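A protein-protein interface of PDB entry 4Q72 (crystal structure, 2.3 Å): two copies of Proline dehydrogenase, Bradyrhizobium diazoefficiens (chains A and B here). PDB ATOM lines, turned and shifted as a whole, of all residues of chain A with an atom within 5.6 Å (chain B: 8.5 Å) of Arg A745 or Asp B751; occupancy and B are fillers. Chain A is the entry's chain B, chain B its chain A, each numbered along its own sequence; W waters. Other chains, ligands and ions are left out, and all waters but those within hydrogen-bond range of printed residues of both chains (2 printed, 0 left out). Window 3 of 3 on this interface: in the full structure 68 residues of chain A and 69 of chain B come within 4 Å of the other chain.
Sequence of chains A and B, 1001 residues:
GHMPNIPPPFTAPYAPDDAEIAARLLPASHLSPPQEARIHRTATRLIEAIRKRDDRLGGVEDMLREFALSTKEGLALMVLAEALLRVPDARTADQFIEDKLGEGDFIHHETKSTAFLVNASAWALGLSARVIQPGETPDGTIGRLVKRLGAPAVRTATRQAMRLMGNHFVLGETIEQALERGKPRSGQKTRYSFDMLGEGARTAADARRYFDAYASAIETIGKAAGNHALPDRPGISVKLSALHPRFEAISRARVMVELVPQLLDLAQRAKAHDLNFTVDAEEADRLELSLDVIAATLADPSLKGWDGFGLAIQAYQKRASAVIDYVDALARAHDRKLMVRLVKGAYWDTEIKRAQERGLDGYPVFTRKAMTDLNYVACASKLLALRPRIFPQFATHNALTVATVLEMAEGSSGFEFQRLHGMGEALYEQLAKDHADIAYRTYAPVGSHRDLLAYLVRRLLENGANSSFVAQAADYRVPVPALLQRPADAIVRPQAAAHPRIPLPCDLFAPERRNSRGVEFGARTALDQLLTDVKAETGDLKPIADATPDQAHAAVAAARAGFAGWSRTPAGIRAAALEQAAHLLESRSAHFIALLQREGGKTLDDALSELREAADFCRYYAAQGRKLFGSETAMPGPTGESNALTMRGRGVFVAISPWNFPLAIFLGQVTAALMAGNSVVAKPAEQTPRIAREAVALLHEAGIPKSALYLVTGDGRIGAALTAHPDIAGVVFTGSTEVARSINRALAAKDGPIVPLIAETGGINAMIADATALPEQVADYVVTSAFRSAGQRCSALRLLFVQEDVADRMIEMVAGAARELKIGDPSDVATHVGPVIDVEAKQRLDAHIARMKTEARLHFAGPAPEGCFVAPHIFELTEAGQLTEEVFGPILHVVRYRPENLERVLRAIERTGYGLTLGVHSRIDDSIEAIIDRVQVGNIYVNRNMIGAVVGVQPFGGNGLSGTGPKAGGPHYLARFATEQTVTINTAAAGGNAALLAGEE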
ATOM      1  N   ALA A 740      -7.078 -14.481  22.704  1.00  0.00           N
ATOM      2  CA  ALA A 740      -5.953 -15.361  23.013  1.00  0.00           C
ATOM      3  C   ALA A 740      -5.467 -16.091  21.763  1.00  0.00           C
ATOM      4  O   ALA A 740      -4.267 -16.160  21.503  1.00  0.00           O
ATOM      5  CB  ALA A 740      -6.333 -16.354  24.086  1.00  0.00           C
ATOM      6  N   ARG A 741      -6.409 -16.607  20.980  1.00  0.00           N
ATOM      7  CA  ARG A 741      -6.083 -17.269  19.722  1.00  0.00           C
ATOM      8  C   ARG A 741      -5.409 -16.348  18.732  1.00  0.00           C
ATOM      9  O   ARG A 741      -4.461 -16.754  18.055  1.00  0.00           O
ATOM     10  CB  ARG A 741      -7.333 -17.836  19.063  1.00  0.00           C
ATOM     11  CG  ARG A 741      -7.836 -19.118  19.686  1.00  0.00           C
ATOM     12  CD  ARG A 741      -8.790 -19.780  18.716  1.00  0.00           C
ATOM     13  NE  ARG A 741      -9.982 -18.967  18.481  1.00  0.00           N
ATOM     14  CZ  ARG A 741     -11.081 -19.081  19.215  1.00  0.00           C
ATOM     15  NH1 ARG A 741     -11.102 -19.964  20.201  1.00  0.00           N
ATOM     16  NH2 ARG A 741     -12.143 -18.325  18.975  1.00  0.00           N
ATOM     17  N   SER A 742      -5.900 -15.116  18.636  1.00  0.00           N
ATOM     18  CA  SER A 742      -5.316 -14.168  17.701  1.00  0.00           C
ATOM     19  C   SER A 742      -3.884 -13.797  18.151  1.00  0.00           C
ATOM     20  O   SER A 742      -2.956 -13.772  17.328  1.00  0.00           O
ATOM     21  CB  SER A 742      -6.228 -12.944  17.519  1.00  0.00           C
ATOM     22  OG  SER A 742      -6.077 -12.007  18.570  1.00  0.00           O
ATOM     23  N   ILE A 743      -3.696 -13.568  19.453  1.00  0.00           N
ATOM     24  CA  ILE A 743      -2.347 -13.405  20.022  1.00  0.00           C
ATOM     25  C   ILE A 743      -1.464 -14.621  19.722  1.00  0.00           C
ATOM     26  O   ILE A 743      -0.343 -14.472  19.252  1.00  0.00           O
ATOM     27  CB  ILE A 743      -2.382 -13.185  21.543  1.00  0.00           C
ATOM     28  CG1 ILE A 743      -2.951 -11.803  21.871  1.00  0.00           C
ATOM     29  CG2 ILE A 743      -0.989 -13.355  22.154  1.00  0.00           C
ATOM     30  CD1 ILE A 743      -3.209 -11.578  23.359  1.00  0.00           C
ATOM     31  N   ASN A 744      -1.992 -15.815  19.971  1.00  0.00           N
ATOM     32  CA  ASN A 744      -1.263 -17.050  19.717  1.00  0.00           C
ATOM     33  C   ASN A 744      -0.876 -17.190  18.246  1.00  0.00           C
ATOM     34  O   ASN A 744       0.199 -17.696  17.922  1.00  0.00           O
ATOM     35  CB  ASN A 744      -2.093 -18.258  20.155  1.00  0.00           C
ATOM     36  CG  ASN A 744      -1.271 -19.543  20.246  1.00  0.00           C
ATOM     37  OD1 ASN A 744      -0.106 -19.538  20.671  1.00  0.00           O
ATOM     38  ND2 ASN A 744      -1.879 -20.658  19.831  1.00  0.00           N
ATOM     39  N   ARG A 745      -1.745 -16.715  17.357  1.00  0.00           N
ATOM     40  CA  ARG A 745      -1.483 -16.789  15.920  1.00  0.00           C
ATOM     41  C   ARG A 745      -0.420 -15.804  15.491  1.00  0.00           C
ATOM     42  O   ARG A 745       0.434 -16.120  14.655  1.00  0.00           O
ATOM     43  CB  ARG A 745      -2.756 -16.546  15.122  1.00  0.00           C
ATOM     44  CG  ARG A 745      -3.550 -17.823  14.906  1.00  0.00           C
ATOM     45  CD  ARG A 745      -5.023 -17.594  14.637  1.00  0.00           C
ATOM     46  NE  ARG A 745      -5.753 -18.777  15.074  1.00  0.00           N
ATOM     47  CZ  ARG A 745      -7.073 -18.860  15.161  1.00  0.00           C
ATOM     48  NH1 ARG A 745      -7.634 -19.987  15.594  1.00  0.00           N
ATOM     49  NH2 ARG A 745      -7.826 -17.818  14.816  1.00  0.00           N
ATOM     50  N   ALA A 746      -0.494 -14.600  16.050  1.00  0.00           N
ATOM     51  CA  ALA A 746       0.500 -13.572  15.776  1.00  0.00           C
ATOM     52  C   ALA A 746       1.883 -14.009  16.272  1.00  0.00           C
ATOM     53  O   ALA A 746       2.880 -13.712  15.636  1.00  0.00           O
ATOM     54  CB  ALA A 746       0.090 -12.233  16.383  1.00  0.00           C
ATOM     55  N   LEU A 747       1.943 -14.728  17.390  1.00  0.00           N
ATOM     56  CA  LEU A 747       3.232 -15.238  17.868  1.00  0.00           C
ATOM     57  C   LEU A 747       3.784 -16.322  16.933  1.00  0.00           C
ATOM     58  O   LEU A 747       4.951 -16.265  16.528  1.00  0.00           O
ATOM     59  CB  LEU A 747       3.115 -15.757  19.312  1.00  0.00           C
ATOM     60  CG  LEU A 747       2.775 -14.660  20.329  1.00  0.00           C
ATOM     61  CD1 LEU A 747       2.467 -15.239  21.699  1.00  0.00           C
ATOM     62  CD2 LEU A 747       3.911 -13.663  20.428  1.00  0.00           C
ATOM     63  N   ALA A 748       2.949 -17.286  16.554  1.00  0.00           N
ATOM     64  CA  ALA A 748       3.429 -18.375  15.714  1.00  0.00           C
ATOM     65  C   ALA A 748       3.826 -17.881  14.321  1.00  0.00           C
ATOM     66  O   ALA A 748       4.651 -18.496  13.640  1.00  0.00           O
ATOM     67  CB  ALA A 748       2.386 -19.473  15.612  1.00  0.00           C
ATOM     68  N   ALA A 749       3.260 -16.750  13.921  1.00  0.00           N
ATOM     69  CA  ALA A 749       3.518 -16.204  12.603  1.00  0.00           C
ATOM     70  C   ALA A 749       4.942 -15.666  12.489  1.00  0.00           C
ATOM     71  O   ALA A 749       5.516 -15.666  11.402  1.00  0.00           O
ATOM     72  CB  ALA A 749       2.491 -15.109  12.269  1.00  0.00           C
ATOM     73  N   LYS A 750       5.508 -15.199  13.601  1.00  0.00           N
ATOM     74  CA  LYS A 750       6.873 -14.658  13.602  1.00  0.00           C
ATOM     75  C   LYS A 750       7.900 -15.708  13.200  1.00  0.00           C
ATOM     76  O   LYS A 750       7.678 -16.911  13.394  1.00  0.00           O
ATOM     77  CB  LYS A 750       7.253 -14.135  14.981  1.00  0.00           C
ATOM     78  CG  LYS A 750       6.387 -13.034  15.518  1.00  0.00           C
ATOM     79  CD  LYS A 750       6.726 -12.799  16.976  1.00  0.00           C
ATOM     80  CE  LYS A 750       5.912 -11.670  17.557  1.00  0.00           C
ATOM     81  NZ  LYS A 750       6.214 -11.495  19.006  1.00  0.00           N
ATOM     82  N   LEU A 961     -10.515 -24.982  26.503  1.00  0.00           N
ATOM     83  CA  LEU A 961     -10.794 -23.621  26.053  1.00  0.00           C
ATOM     84  C   LEU A 961     -10.643 -22.562  27.152  1.00  0.00           C
ATOM     85  O   LEU A 961     -10.683 -21.365  26.879  1.00  0.00           O
ATOM     86  CB  LEU A 961     -12.211 -23.533  25.448  1.00  0.00           C
ATOM     87  CG  LEU A 961     -12.546 -24.385  24.226  1.00  0.00           C
ATOM     88  CD1 LEU A 961     -13.960 -24.094  23.697  1.00  0.00           C
ATOM     89  CD2 LEU A 961     -11.540 -24.111  23.140  1.00  0.00           C
ATOM     90  N   ALA B 724      -2.066 -31.599  13.101  1.00  0.00           N
ATOM     91  CA  ALA B 724      -3.207 -30.798  12.687  1.00  0.00           C
ATOM     92  C   ALA B 724      -4.508 -31.364  13.254  1.00  0.00           C
ATOM     93  O   ALA B 724      -5.527 -30.690  13.242  1.00  0.00           O
ATOM     94  CB  ALA B 724      -3.276 -30.686  11.156  1.00  0.00           C
ATOM     95  N   PRO B 726      -7.606 -32.188  15.372  1.00  0.00           N
ATOM     96  CA  PRO B 726      -8.304 -31.360  16.369  1.00  0.00           C
ATOM     97  C   PRO B 726      -8.354 -31.928  17.789  1.00  0.00           C
ATOM     98  O   PRO B 726      -8.566 -31.141  18.719  1.00  0.00           O
ATOM     99  CB  PRO B 726      -9.734 -31.247  15.799  1.00  0.00           C
ATOM    100  CG  PRO B 726      -9.888 -32.430  14.884  1.00  0.00           C
ATOM    101  CD  PRO B 726      -8.507 -32.603  14.276  1.00  0.00           C
ATOM    102  N   ASN B 744       4.016 -25.230  15.056  1.00  0.00           N
ATOM    103  CA  ASN B 744       3.477 -24.198  15.930  1.00  0.00           C
ATOM    104  C   ASN B 744       2.381 -23.402  15.227  1.00  0.00           C
ATOM    105  O   ASN B 744       1.367 -23.052  15.834  1.00  0.00           O
ATOM    106  CB  ASN B 744       4.603 -23.274  16.406  1.00  0.00           C
ATOM    107  CG  ASN B 744       4.199 -22.420  17.607  1.00  0.00           C
ATOM    108  OD1 ASN B 744       3.455 -22.872  18.494  1.00  0.00           O
ATOM    109  ND2 ASN B 744       4.705 -21.183  17.651  1.00  0.00           N
ATOM    110  N   ARG B 745       2.551 -23.173  13.928  1.00  0.00           N
ATOM    111  CA  ARG B 745       1.547 -22.432  13.165  1.00  0.00           C
ATOM    112  C   ARG B 745       0.290 -23.256  12.952  1.00  0.00           C
ATOM    113  O   ARG B 745      -0.822 -22.732  13.062  1.00  0.00           O
ATOM    114  CB  ARG B 745       2.087 -21.994  11.816  1.00  0.00           C
ATOM    115  CG  ARG B 745       2.823 -20.668  11.878  1.00  0.00           C
ATOM    116  CD  ARG B 745       3.815 -20.495  10.756  1.00  0.00           C
ATOM    117  NE  ARG B 745       4.866 -19.586  11.196  1.00  0.00           N
ATOM    118  CZ  ARG B 745       6.003 -19.368  10.537  1.00  0.00           C
ATOM    119  NH1 ARG B 745       6.912 -18.533  11.039  1.00  0.00           N
ATOM    120  NH2 ARG B 745       6.228 -19.993   9.386  1.00  0.00           N
ATOM    121  N   ALA B 746       0.468 -24.542  12.650  1.00  0.00           N
ATOM    122  CA  ALA B 746      -0.671 -25.434  12.470  1.00  0.00           C
ATOM    123  C   ALA B 746      -1.491 -25.570  13.777  1.00  0.00           C
ATOM    124  O   ALA B 746      -2.703 -25.639  13.742  1.00  0.00           O
ATOM    125  CB  ALA B 746      -0.212 -26.793  11.947  1.00  0.00           C
ATOM    126  N   LEU B 747      -0.827 -25.571  14.929  1.00  0.00           N
ATOM    127  CA  LEU B 747      -1.556 -25.597  16.200  1.00  0.00           C
ATOM    128  C   LEU B 747      -2.315 -24.291  16.468  1.00  0.00           C
ATOM    129  O   LEU B 747      -3.505 -24.308  16.782  1.00  0.00           O
ATOM    130  CB  LEU B 747      -0.596 -25.903  17.348  1.00  0.00           C
ATOM    131  CG  LEU B 747       0.016 -27.303  17.296  1.00  0.00           C
ATOM    132  CD1 LEU B 747       1.135 -27.443  18.333  1.00  0.00           C
ATOM    133  CD2 LEU B 747      -1.079 -28.336  17.558  1.00  0.00           C
ATOM    134  N   ALA B 748      -1.641 -23.157  16.299  1.00  0.00           N
ATOM    135  CA  ALA B 748      -2.257 -21.871  16.588  1.00  0.00           C
ATOM    136  C   ALA B 748      -3.411 -21.564  15.630  1.00  0.00           C
ATOM    137  O   ALA B 748      -4.283 -20.746  15.931  1.00  0.00           O
ATOM    138  CB  ALA B 748      -1.230 -20.770  16.544  1.00  0.00           C
ATOM    139  N   ALA B 749      -3.404 -22.221  14.476  1.00  0.00           N
ATOM    140  CA  ALA B 749      -4.447 -22.014  13.489  1.00  0.00           C
ATOM    141  C   ALA B 749      -5.782 -22.622  13.937  1.00  0.00           C
ATOM    142  O   ALA B 749      -6.844 -22.124  13.566  1.00  0.00           O
ATOM    143  CB  ALA B 749      -4.015 -22.585  12.126  1.00  0.00           C
ATOM    144  N   LYS B 750      -5.732 -23.696  14.723  1.00  0.00           N
ATOM    145  CA  LYS B 750      -6.955 -24.365  15.192  1.00  0.00           C
ATOM    146  C   LYS B 750      -7.799 -23.431  16.054  1.00  0.00           C
ATOM    147  O   LYS B 750      -7.259 -22.531  16.718  1.00  0.00           O
ATOM    148  CB  LYS B 750      -6.608 -25.599  16.032  1.00  0.00           C
ATOM    149  CG  LYS B 750      -5.746 -26.637  15.329  1.00  0.00           C
ATOM    150  CD  LYS B 750      -5.260 -27.689  16.312  1.00  0.00           C
ATOM    151  CE  LYS B 750      -4.472 -28.782  15.620  1.00  0.00           C
ATOM    152  NZ  LYS B 750      -3.962 -29.799  16.594  1.00  0.00           N
ATOM    153  N   ASP B 751      -9.113 -23.664  16.071  1.00  0.00           N
ATOM    154  CA  ASP B 751     -10.015 -22.895  16.921  1.00  0.00           C
ATOM    155  C   ASP B 751     -10.159 -23.554  18.281  1.00  0.00           C
ATOM    156  O   ASP B 751     -10.776 -22.995  19.187  1.00  0.00           O
ATOM    157  CB  ASP B 751     -11.395 -22.715  16.277  1.00  0.00           C
ATOM    158  CG  ASP B 751     -11.325 -22.007  14.940  1.00  0.00           C
ATOM    159  OD1 ASP B 751     -11.128 -20.768  14.931  1.00  0.00           O
ATOM    160  OD2 ASP B 751     -11.477 -22.683  13.901  1.00  0.00           O
ATOM    161  N   GLY B 752      -9.627 -24.761  18.415  1.00  0.00           N
ATOM    162  CA  GLY B 752      -9.703 -25.459  19.683  1.00  0.00           C
ATOM    163  C   GLY B 752      -8.851 -24.854  20.793  1.00  0.00           C
ATOM    164  O   GLY B 752      -8.446 -23.684  20.727  1.00  0.00           O
ATOM    165  N   PRO B 753      -8.580 -25.656  21.835  1.00  0.00           N
ATOM    166  CA  PRO B 753      -7.688 -25.270  22.931  1.00  0.00           C
ATOM    167  C   PRO B 753      -6.280 -24.990  22.418  1.00  0.00           C
ATOM    168  O   PRO B 753      -5.870 -25.583  21.415  1.00  0.00           O
ATOM    169  CB  PRO B 753      -7.644 -26.524  23.798  1.00  0.00           C
ATOM    170  CG  PRO B 753      -8.919 -27.232  23.492  1.00  0.00           C
ATOM    171  CD  PRO B 753      -9.173 -26.984  22.044  1.00  0.00           C
ATOM    172  N   ILE B 754      -5.589 -24.063  23.077  1.00  0.00           N
ATOM    173  CA  ILE B 754      -4.163 -23.813  22.856  1.00  0.00           C
ATOM    174  C   ILE B 754      -3.459 -24.905  23.623  1.00  0.00           C
ATOM    175  O   ILE B 754      -3.587 -24.979  24.837  1.00  0.00           O
ATOM    176  CB  ILE B 754      -3.730 -22.425  23.384  1.00  0.00           C
ATOM    177  CG1 ILE B 754      -4.435 -21.317  22.602  1.00  0.00           C
ATOM    178  CG2 ILE B 754      -2.192 -22.237  23.317  1.00  0.00           C
ATOM    179  CD1 ILE B 754      -4.331 -19.944  23.225  1.00  0.00           C
HETATM  180  O   HOH W   1      -4.607 -20.384  18.690  1.00  0.00           O
HETATM  181  O   HOH W   2      -8.952 -21.329  22.317  1.00  0.00           O
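Asn A744 touches Ala B748, and with the chains exchanged Ala A748 touches Asn B744.
Arg A745 touches Ala B748, and with the chains exchanged Ala A748 touches Arg B745.
Arg A745 touches Lys B750, and with the chains exchanged Lys A750 touches Arg B745.
Ala A748 touches its own counterpart, Ala B748.
Of the 15 pairs that touch across the chains among the printed residues, 9 have their exchanged pair printed and touching as well.
Of the 13 printed residues of chain B, 9 touch a printed residue of chain A.
Printed residues of chain B that touch a printed residue of chain A: Asn B744, Arg B745, Ala B748, Ala B749, Lys B750, Asp B751, Gly B752, Pro B753 and Ile B754.
Hydrophobic or aromatic side chains of chain B within 4 Å of the printed part of chain A: Ala B748, Pro B753 and Ile B754.
Of the 12 printed residues of chain A, 7 touch a printed residue of chain B.
Among the printed residues, Asp or Glu carboxylates within 4 Å of a Lys or Arg side-chain nitrogen of the other chain: Arg A745 with Asp B751 (3.6 Å).
Ile A743 touches none of the printed residues of chain B.
No residue of chain B comes within 4 Å of Ala A746.
Leu A747 touches none of the printed residues of chain B.
Of chain A, only Arg A741 (3.2 Å) and Arg A745 (3.6 Å) come within 4 Å of Asp B751.
Of the printed residues of chain A, Pro B753 touches Leu A961 (3.6 Å).
Of the printed residues of chain A, Ile B754 touches Asn A744.
Water W1 lies within hydrogen-bond range of the backbone carbonyl oxygen of Ala B748 (2.8 Å) and the side-chain amide nitrogen of Asn A744 (3.0 Å).
Water W2 bridges O of Gly B752 (2.9 Å) and NH1 of Arg A741 (3.3 Å).
Among the printed residues, pairs that only touch across the chains: Asn A744 with Ala B748, Ala A748 with Asn B744, Leu A961 with Pro B753, Leu A961 with Gly B752, Arg A741 with Lys B750, Asn A744 with Ile B754 and Ala A748 with Ala B748.
The backbone carbonyl oxygen (O) of Ala A748 sits at hydrogen-bond distance from the guanidinium group (NE) of Arg B745.
NH1 of Arg B745 lies within hydrogen-bond range of O of Ala A749 (3.2 Å).
NH1 of Arg B745 lies within hydrogen-bond range of O of Lys A750 (3.0 Å).
The backbone carbonyl oxygen (O) of Ala B748 sits at hydrogen-bond distance from the guanidinium group (NE) of Arg A745.
O of Ala B749 lies within hydrogen-bond range of NH1 of Arg A745 (3.1 Å).
The backbone carbonyl oxygen (O) of Lys B750 sits at hydrogen-bond distance from the guanidinium group (NH1) of Arg A745, at 2.8 Å.
The guanidinium group of Arg A741 is in hydrogen-bond range of the backbone carbonyl oxygen of Asp B751 (3.2 Å).
OD1 of Asp B751 lies within salt-bridge range of NH1 of Arg A745, 3.6 Å away.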
